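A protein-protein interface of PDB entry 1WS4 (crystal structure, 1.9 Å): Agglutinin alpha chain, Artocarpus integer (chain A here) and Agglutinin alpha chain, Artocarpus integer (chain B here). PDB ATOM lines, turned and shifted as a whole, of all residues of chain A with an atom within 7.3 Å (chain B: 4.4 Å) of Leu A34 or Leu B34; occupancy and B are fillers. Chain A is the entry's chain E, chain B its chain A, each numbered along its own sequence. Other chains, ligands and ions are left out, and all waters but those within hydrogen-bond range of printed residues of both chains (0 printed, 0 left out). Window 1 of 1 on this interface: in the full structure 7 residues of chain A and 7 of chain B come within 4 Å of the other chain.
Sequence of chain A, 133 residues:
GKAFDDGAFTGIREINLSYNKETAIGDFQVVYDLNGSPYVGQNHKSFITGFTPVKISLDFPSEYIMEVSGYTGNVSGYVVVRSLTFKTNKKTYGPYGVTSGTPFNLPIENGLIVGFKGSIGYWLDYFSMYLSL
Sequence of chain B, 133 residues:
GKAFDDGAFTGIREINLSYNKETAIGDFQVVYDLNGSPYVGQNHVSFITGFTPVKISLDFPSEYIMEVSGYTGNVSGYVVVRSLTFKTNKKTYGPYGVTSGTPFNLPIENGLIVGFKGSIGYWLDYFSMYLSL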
ATOM      1  N   ASP A   6     -23.376  17.749  18.943  1.00  0.00           N
ATOM      2  CA  ASP A   6     -23.155  19.126  19.379  1.00  0.00           C
ATOM      3  C   ASP A   6     -24.382  20.003  19.151  1.00  0.00           C
ATOM      4  O   ASP A   6     -24.637  20.937  19.910  1.00  0.00           O
ATOM      5  CB  ASP A   6     -21.966  19.749  18.643  1.00  0.00           C
ATOM      6  CG  ASP A   6     -20.631  19.217  19.125  1.00  0.00           C
ATOM      7  OD1 ASP A   6     -20.586  18.580  20.198  1.00  0.00           O
ATOM      8  OD2 ASP A   6     -19.623  19.453  18.430  1.00  0.00           O
ATOM      9  N   GLY A   7     -25.139  19.707  18.104  1.00  0.00           N
ATOM     10  CA  GLY A   7     -26.312  20.509  17.812  1.00  0.00           C
ATOM     11  C   GLY A   7     -25.955  21.584  16.806  1.00  0.00           C
ATOM     12  O   GLY A   7     -24.858  21.573  16.249  1.00  0.00           O
ATOM     13  N   ALA A   8     -26.866  22.526  16.587  1.00  0.00           N
ATOM     14  CA  ALA A   8     -26.633  23.589  15.621  1.00  0.00           C
ATOM     15  C   ALA A   8     -26.316  24.928  16.275  1.00  0.00           C
ATOM     16  O   ALA A   8     -26.901  25.288  17.297  1.00  0.00           O
ATOM     17  CB  ALA A   8     -27.850  23.731  14.712  1.00  0.00           C
ATOM     18  N   PHE A   9     -25.386  25.660  15.672  1.00  0.00           N
ATOM     19  CA  PHE A   9     -24.986  26.970  16.164  1.00  0.00           C
ATOM     20  C   PHE A   9     -25.081  27.978  15.021  1.00  0.00           C
ATOM     21  O   PHE A   9     -25.745  27.714  14.028  1.00  0.00           O
ATOM     22  CB  PHE A   9     -23.567  26.907  16.733  1.00  0.00           C
ATOM     23  CG  PHE A   9     -23.447  26.011  17.928  1.00  0.00           C
ATOM     24  CD1 PHE A   9     -23.370  24.629  17.775  1.00  0.00           C
ATOM     25  CD2 PHE A   9     -23.474  26.541  19.213  1.00  0.00           C
ATOM     26  CE1 PHE A   9     -23.321  23.790  18.885  1.00  0.00           C
ATOM     27  CE2 PHE A   9     -23.428  25.711  20.331  1.00  0.00           C
ATOM     28  CZ  PHE A   9     -23.351  24.331  20.167  1.00  0.00           C
ATOM     29  N   THR A  10     -24.427  29.128  15.142  1.00  0.00           N
ATOM     30  CA  THR A  10     -24.518  30.120  14.077  1.00  0.00           C
ATOM     31  C   THR A  10     -23.301  30.194  13.164  1.00  0.00           C
ATOM     32  O   THR A  10     -23.302  30.938  12.187  1.00  0.00           O
ATOM     33  CB  THR A  10     -24.836  31.525  14.651  1.00  0.00           C
ATOM     34  OG1 THR A  10     -23.925  31.840  15.706  1.00  0.00           O
ATOM     35  CG2 THR A  10     -26.260  31.558  15.203  1.00  0.00           C
ATOM     36  N   GLY A  11     -22.274  29.407  13.470  1.00  0.00           N
ATOM     37  CA  GLY A  11     -21.078  29.403  12.646  1.00  0.00           C
ATOM     38  C   GLY A  11     -19.976  28.572  13.276  1.00  0.00           C
ATOM     39  O   GLY A  11     -20.160  28.002  14.351  1.00  0.00           O
ATOM     40  N   ILE A  12     -18.829  28.504  12.608  1.00  0.00           N
ATOM     41  CA  ILE A  12     -17.696  27.740  13.112  1.00  0.00           C
ATOM     42  C   ILE A  12     -16.451  28.619  13.203  1.00  0.00           C
ATOM     43  O   ILE A  12     -16.118  29.340  12.263  1.00  0.00           O
ATOM     44  CB  ILE A  12     -17.397  26.536  12.195  1.00  0.00           C
ATOM     45  CG1 ILE A  12     -18.619  25.611  12.140  1.00  0.00           C
ATOM     46  CG2 ILE A  12     -16.192  25.764  12.724  1.00  0.00           C
ATOM     47  CD1 ILE A  12     -18.479  24.478  11.155  1.00  0.00           C
ATOM     48  N   ARG A  13     -15.766  28.552  14.338  1.00  0.00           N
ATOM     49  CA  ARG A  13     -14.562  29.348  14.540  1.00  0.00           C
ATOM     50  C   ARG A  13     -13.279  28.527  14.493  1.00  0.00           C
ATOM     51  O   ARG A  13     -12.293  28.945  13.887  1.00  0.00           O
ATOM     52  CB  ARG A  13     -14.643  30.085  15.882  1.00  0.00           C
ATOM     53  CG  ARG A  13     -15.610  31.263  15.882  1.00  0.00           C
ATOM     54  CD  ARG A  13     -15.898  31.756  17.292  1.00  0.00           C
ATOM     55  NE  ARG A  13     -16.742  32.949  17.289  1.00  0.00           N
ATOM     56  CZ  ARG A  13     -16.281  34.198  17.240  1.00  0.00           C
ATOM     57  NH1 ARG A  13     -14.975  34.429  17.197  1.00  0.00           N
ATOM     58  NH2 ARG A  13     -17.130  35.218  17.234  1.00  0.00           N
ATOM     59  N   VAL A  31     -15.010  24.674  18.173  1.00  0.00           N
ATOM     60  CA  VAL A  31     -15.322  25.926  18.850  1.00  0.00           C
ATOM     61  C   VAL A  31     -16.287  26.592  17.873  1.00  0.00           C
ATOM     62  O   VAL A  31     -15.908  26.965  16.766  1.00  0.00           O
ATOM     63  CB  VAL A  31     -14.088  26.829  19.052  1.00  0.00           C
ATOM     64  CG1 VAL A  31     -14.513  28.135  19.733  1.00  0.00           C
ATOM     65  CG2 VAL A  31     -13.060  26.116  19.916  1.00  0.00           C
ATOM     66  N   TYR A  32     -17.546  26.695  18.273  1.00  0.00           N
ATOM     67  CA  TYR A  32     -18.562  27.288  17.421  1.00  0.00           C
ATOM     68  C   TYR A  32     -18.752  28.749  17.733  1.00  0.00           C
ATOM     69  O   TYR A  32     -18.268  29.250  18.749  1.00  0.00           O
ATOM     70  CB  TYR A  32     -19.921  26.618  17.643  1.00  0.00           C
ATOM     71  CG  TYR A  32     -19.966  25.146  17.341  1.00  0.00           C
ATOM     72  CD1 TYR A  32     -19.775  24.198  18.349  1.00  0.00           C
ATOM     73  CD2 TYR A  32     -20.194  24.696  16.042  1.00  0.00           C
ATOM     74  CE1 TYR A  32     -19.813  22.834  18.067  1.00  0.00           C
ATOM     75  CE2 TYR A  32     -20.230  23.339  15.748  1.00  0.00           C
ATOM     76  CZ  TYR A  32     -20.040  22.416  16.760  1.00  0.00           C
ATOM     77  OH  TYR A  32     -20.085  21.076  16.461  1.00  0.00           O
ATOM     78  N   ASP A  33     -19.461  29.428  16.840  1.00  0.00           N
ATOM     79  CA  ASP A  33     -19.816  30.810  17.079  1.00  0.00           C
ATOM     80  C   ASP A  33     -21.261  30.700  17.536  1.00  0.00           C
ATOM     81  O   ASP A  33     -22.033  29.922  16.981  1.00  0.00           O
ATOM     82  CB  ASP A  33     -19.779  31.654  15.810  1.00  0.00           C
ATOM     83  CG  ASP A  33     -20.267  33.072  16.059  1.00  0.00           C
ATOM     84  OD1 ASP A  33     -19.541  33.833  16.732  1.00  0.00           O
ATOM     85  OD2 ASP A  33     -21.381  33.416  15.605  1.00  0.00           O
ATOM     86  N   LEU A  34     -21.620  31.454  18.565  1.00  0.00           N
ATOM     87  CA  LEU A  34     -22.985  31.449  19.056  1.00  0.00           C
ATOM     88  C   LEU A  34     -23.430  32.900  19.129  1.00  0.00           C
ATOM     89  O   LEU A  34     -23.153  33.597  20.107  1.00  0.00           O
ATOM     90  CB  LEU A  34     -23.078  30.806  20.440  1.00  0.00           C
ATOM     91  CG  LEU A  34     -24.491  30.794  21.037  1.00  0.00           C
ATOM     92  CD1 LEU A  34     -25.454  30.072  20.100  1.00  0.00           C
ATOM     93  CD2 LEU A  34     -24.463  30.120  22.389  1.00  0.00           C
ATOM     94  N   ASN A  35     -24.094  33.350  18.071  1.00  0.00           N
ATOM     95  CA  ASN A  35     -24.589  34.713  17.998  1.00  0.00           C
ATOM     96  C   ASN A  35     -23.488  35.752  18.233  1.00  0.00           C
ATOM     97  O   ASN A  35     -23.683  36.717  18.969  1.00  0.00           O
ATOM     98  CB  ASN A  35     -25.720  34.889  19.016  1.00  0.00           C
ATOM     99  CG  ASN A  35     -26.858  33.907  18.791  1.00  0.00           C
ATOM    100  OD1 ASN A  35     -27.309  33.235  19.723  1.00  0.00           O
ATOM    101  ND2 ASN A  35     -27.329  33.821  17.552  1.00  0.00           N
ATOM    102  N   GLY A  36     -22.328  35.544  17.614  1.00  0.00           N
ATOM    103  CA  GLY A  36     -21.238  36.496  17.753  1.00  0.00           C
ATOM    104  C   GLY A  36     -20.198  36.210  18.818  1.00  0.00           C
ATOM    105  O   GLY A  36     -19.163  36.878  18.865  1.00  0.00           O
ATOM    106  N   SER A  37     -20.465  35.237  19.681  1.00  0.00           N
ATOM    107  CA  SER A  37     -19.524  34.878  20.734  1.00  0.00           C
ATOM    108  C   SER A  37     -19.057  33.439  20.571  1.00  0.00           C
ATOM    109  O   SER A  37     -19.813  32.578  20.120  1.00  0.00           O
ATOM    110  CB  SER A  37     -20.164  35.035  22.116  1.00  0.00           C
ATOM    111  OG  SER A  37     -20.332  36.401  22.459  1.00  0.00           O
ATOM    112  N   PRO A  38     -17.794  33.164  20.924  1.00  0.00           N
ATOM    113  CA  PRO A  38     -17.261  31.804  20.808  1.00  0.00           C
ATOM    114  C   PRO A  38     -17.949  30.867  21.798  1.00  0.00           C
ATOM    115  O   PRO A  38     -18.237  31.255  22.931  1.00  0.00           O
ATOM    116  CB  PRO A  38     -15.778  31.981  21.142  1.00  0.00           C
ATOM    117  CG  PRO A  38     -15.498  33.406  20.749  1.00  0.00           C
ATOM    118  CD  PRO A  38     -16.725  34.122  21.258  1.00  0.00           C
ATOM    119  N   TYR A  39     -18.226  29.644  21.363  1.00  0.00           N
ATOM    120  CA  TYR A  39     -18.839  28.648  22.233  1.00  0.00           C
ATOM    121  C   TYR A  39     -18.017  27.372  22.089  1.00  0.00           C
ATOM    122  O   TYR A  39     -17.990  26.762  21.021  1.00  0.00           O
ATOM    123  CB  TYR A  39     -20.296  28.387  21.838  1.00  0.00           C
ATOM    124  CG  TYR A  39     -20.984  27.385  22.737  1.00  0.00           C
ATOM    125  CD1 TYR A  39     -20.797  26.015  22.559  1.00  0.00           C
ATOM    126  CD2 TYR A  39     -21.787  27.809  23.794  1.00  0.00           C
ATOM    127  CE1 TYR A  39     -21.394  25.090  23.412  1.00  0.00           C
ATOM    128  CE2 TYR A  39     -22.386  26.892  24.655  1.00  0.00           C
ATOM    129  CZ  TYR A  39     -22.185  25.537  24.459  1.00  0.00           C
ATOM    130  OH  TYR A  39     -22.770  24.629  25.309  1.00  0.00           O
ATOM    131  N   PHE A  60     -12.905  33.637  11.193  1.00  0.00           N
ATOM    132  CA  PHE A  60     -14.333  33.923  11.271  1.00  0.00           C
ATOM    133  C   PHE A  60     -14.521  35.441  11.344  1.00  0.00           C
ATOM    134  O   PHE A  60     -13.772  36.130  12.038  1.00  0.00           O
ATOM    135  CB  PHE A  60     -14.907  33.258  12.528  1.00  0.00           C
ATOM    136  CG  PHE A  60     -16.388  33.437  12.698  1.00  0.00           C
ATOM    137  CD1 PHE A  60     -17.285  32.685  11.947  1.00  0.00           C
ATOM    138  CD2 PHE A  60     -16.889  34.354  13.615  1.00  0.00           C
ATOM    139  CE1 PHE A  60     -18.657  32.844  12.108  1.00  0.00           C
ATOM    140  CE2 PHE A  60     -18.259  34.521  13.782  1.00  0.00           C
ATOM    141  CZ  PHE A  60     -19.145  33.763  13.025  1.00  0.00           C
ATOM    142  N   PHE B   9     -31.639  30.698  19.059  1.00  0.00           N
ATOM    143  CA  PHE B   9     -31.355  29.489  19.820  1.00  0.00           C
ATOM    144  C   PHE B   9     -32.182  28.299  19.342  1.00  0.00           C
ATOM    145  O   PHE B   9     -32.756  28.330  18.254  1.00  0.00           O
ATOM    146  CB  PHE B   9     -31.588  29.747  21.312  1.00  0.00           C
ATOM    147  CG  PHE B   9     -30.652  30.765  21.890  1.00  0.00           C
ATOM    148  CD1 PHE B   9     -30.887  32.125  21.717  1.00  0.00           C
ATOM    149  CD2 PHE B   9     -29.498  30.365  22.557  1.00  0.00           C
ATOM    150  CE1 PHE B   9     -29.987  33.072  22.200  1.00  0.00           C
ATOM    151  CE2 PHE B   9     -28.592  31.305  23.042  1.00  0.00           C
ATOM    152  CZ  PHE B   9     -28.839  32.662  22.861  1.00  0.00           C
ATOM    153  N   THR B  10     -32.239  27.252  20.161  1.00  0.00           N
ATOM    154  CA  THR B  10     -32.967  26.028  19.820  1.00  0.00           C
ATOM    155  C   THR B  10     -34.429  26.047  20.248  1.00  0.00           C
ATOM    156  O   THR B  10     -35.257  25.324  19.691  1.00  0.00           O
ATOM    157  CB  THR B  10     -32.308  24.797  20.486  1.00  0.00           C
ATOM    158  OG1 THR B  10     -30.903  24.802  20.217  1.00  0.00           O
ATOM    159  CG2 THR B  10     -32.916  23.513  19.946  1.00  0.00           C
ATOM    160  N   TYR B  32     -33.031  30.302  27.276  1.00  0.00           N
ATOM    161  CA  TYR B  32     -33.242  29.576  26.033  1.00  0.00           C
ATOM    162  C   TYR B  32     -32.790  28.136  26.146  1.00  0.00           C
ATOM    163  O   TYR B  32     -32.155  27.742  27.125  1.00  0.00           O
ATOM    164  CB  TYR B  32     -32.435  30.201  24.890  1.00  0.00           C
ATOM    165  CG  TYR B  32     -32.787  31.628  24.553  1.00  0.00           C
ATOM    166  CD1 TYR B  32     -32.110  32.701  25.141  1.00  0.00           C
ATOM    167  CD2 TYR B  32     -33.802  31.906  23.644  1.00  0.00           C
ATOM    168  CE1 TYR B  32     -32.443  34.019  24.822  1.00  0.00           C
ATOM    169  CE2 TYR B  32     -34.143  33.208  23.323  1.00  0.00           C
ATOM    170  CZ  TYR B  32     -33.466  34.258  23.912  1.00  0.00           C
ATOM    171  OH  TYR B  32     -33.837  35.539  23.586  1.00  0.00           O
ATOM    172  N   ASP B  33     -33.138  27.345  25.138  1.00  0.00           N
ATOM    173  CA  ASP B  33     -32.655  25.982  25.088  1.00  0.00           C
ATOM    174  C   ASP B  33     -31.569  26.069  24.034  1.00  0.00           C
ATOM    175  O   ASP B  33     -31.745  26.727  23.008  1.00  0.00           O
ATOM    176  CB  ASP B  33     -33.703  24.985  24.605  1.00  0.00           C
ATOM    177  CG  ASP B  33     -33.128  23.578  24.488  1.00  0.00           C
ATOM    178  OD1 ASP B  33     -32.813  22.980  25.538  1.00  0.00           O
ATOM    179  OD2 ASP B  33     -32.963  23.083  23.351  1.00  0.00           O
ATOM    180  N   LEU B  34     -30.437  25.439  24.299  1.00  0.00           N
ATOM    181  CA  LEU B  34     -29.348  25.439  23.344  1.00  0.00           C
ATOM    182  C   LEU B  34     -28.972  23.987  23.129  1.00  0.00           C
ATOM    183  O   LEU B  34     -28.168  23.432  23.871  1.00  0.00           O
ATOM    184  CB  LEU B  34     -28.141  26.222  23.873  1.00  0.00           C
ATOM    185  CG  LEU B  34     -26.925  26.205  22.942  1.00  0.00           C
ATOM    186  CD1 LEU B  34     -27.304  26.787  21.582  1.00  0.00           C
ATOM    187  CD2 LEU B  34     -25.789  26.993  23.564  1.00  0.00           C
ATOM    188  N   ASN B  35     -29.594  23.372  22.130  1.00  0.00           N
ATOM    189  CA  ASN B  35     -29.322  21.982  21.798  1.00  0.00           C
ATOM    190  C   ASN B  35     -29.516  21.029  22.982  1.00  0.00           C
ATOM    191  O   ASN B  35     -28.652  20.199  23.270  1.00  0.00           O
ATOM    192  CB  ASN B  35     -27.898  21.875  21.245  1.00  0.00           C
ATOM    193  CG  ASN B  35     -27.697  22.743  20.018  1.00  0.00           C
ATOM    194  OD1 ASN B  35     -26.764  23.548  19.947  1.00  0.00           O
ATOM    195  ND2 ASN B  35     -28.580  22.586  19.041  1.00  0.00           N
ATOM    196  N   GLY B  36     -30.654  21.162  23.660  1.00  0.00           N
ATOM    197  CA  GLY B  36     -30.964  20.293  24.784  1.00  0.00           C
ATOM    198  C   GLY B  36     -30.539  20.752  26.167  1.00  0.00           C
ATOM    199  O   GLY B  36     -30.894  20.118  27.161  1.00  0.00           O
ATOM    200  N   SER B  37     -29.779  21.839  26.245  1.00  0.00           N
ATOM    201  CA  SER B  37     -29.322  22.357  27.531  1.00  0.00           C
ATOM    202  C   SER B  37     -29.746  23.807  27.720  1.00  0.00           C
ATOM    203  O   SER B  37     -29.789  24.579  26.766  1.00  0.00           O
ATOM    204  CB  SER B  37     -27.798  22.266  27.636  1.00  0.00           C
ATOM    205  OG  SER B  37     -27.363  20.919  27.595  1.00  0.00           O
ATOM    206  N   TYR B  39     -29.716  27.729  28.466  1.00  0.00           N
ATOM    207  CA  TYR B  39     -28.745  28.781  28.217  1.00  0.00           C
ATOM    208  C   TYR B  39     -29.358  30.067  28.750  1.00  0.00           C
ATOM    209  O   TYR B  39     -30.329  30.579  28.196  1.00  0.00           O
ATOM    210  CB  TYR B  39     -28.431  28.916  26.726  1.00  0.00           C
ATOM    211  CG  TYR B  39     -27.399  29.980  26.448  1.00  0.00           C
ATOM    212  CD1 TYR B  39     -27.763  31.320  26.335  1.00  0.00           C
ATOM    213  CD2 TYR B  39     -26.046  29.655  26.354  1.00  0.00           C
ATOM    214  CE1 TYR B  39     -26.804  32.313  26.136  1.00  0.00           C
ATOM    215  CE2 TYR B  39     -25.081  30.636  26.158  1.00  0.00           C
ATOM    216  CZ  TYR B  39     -25.467  31.962  26.052  1.00  0.00           C
ATOM    217  OH  TYR B  39     -24.513  32.937  25.876  1.00  0.00           O
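Leu A34 touches just these residues of chain B: Leu B34 and Tyr B39. Printed residues of chain A within 4 Å of Leu B34: Leu A34 (3.6 Å) and Tyr A39 (3.6 Å). Of the printed residues of chain B, Phe A9 touches Asn B35. Of the printed residues of chain B, Ala A8 touches Asn B35. The nearest residue of chain B that does not touch Leu A34 is Phe B9 (4.3 Å). The nearest residue of chain A that does not touch Leu B34 is Phe A9 (4.2 Å).
The backbone carbonyl oxygen of Asp A6 sits close to the side-chain amide oxygen of Asn B35 (3.4 Å). The backbone NH of Ala A8 lies close to the side-chain amide nitrogen of Asn B35 (3.0 Å).
Of the 9 printed residues of chain B, 4 touch a printed residue of chain A. Printed residues of chain B that touch a printed residue of chain A: Phe B9, Leu B34, Asn B35 and Tyr B39. Hydrophobic or aromatic side chains of chain B within 4 Å of the printed part of chain A: Phe B9, Leu B34 and Tyr B39. Along chain A the printed residues that touch a printed residue of chain B span positions 6 to 39. Among the printed residues, no Asp or Glu carboxylate lies within 4 Å of a Lys or Arg side-chain nitrogen of the other chain.
OG1 of Thr B10 lies within hydrogen-bond range of N of Asn B35, 2.7 Å away. O of Tyr B32 is in hydrogen-bond range of N of Tyr B39 (2.8 Å). OD2 of Asp A6 sits at hydrogen-bond distance from OH of Tyr A32 (2.6 Å). OG1 of Thr A10 lies within hydrogen-bond range of N of Asn A35 (2.8 Å). The backbone carbonyl oxygen of Tyr A32 sits at hydrogen-bond distance from the backbone NH of Tyr A39 (2.6 Å).
Among the printed residues, merely in contact across the chains: Gly A7 with Asn B35, Phe A9 with Asn B35, Asn A35 with Phe B9, Tyr A39 with Leu B34, Leu A34 with Leu B34 and Leu A34 with Tyr B39.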
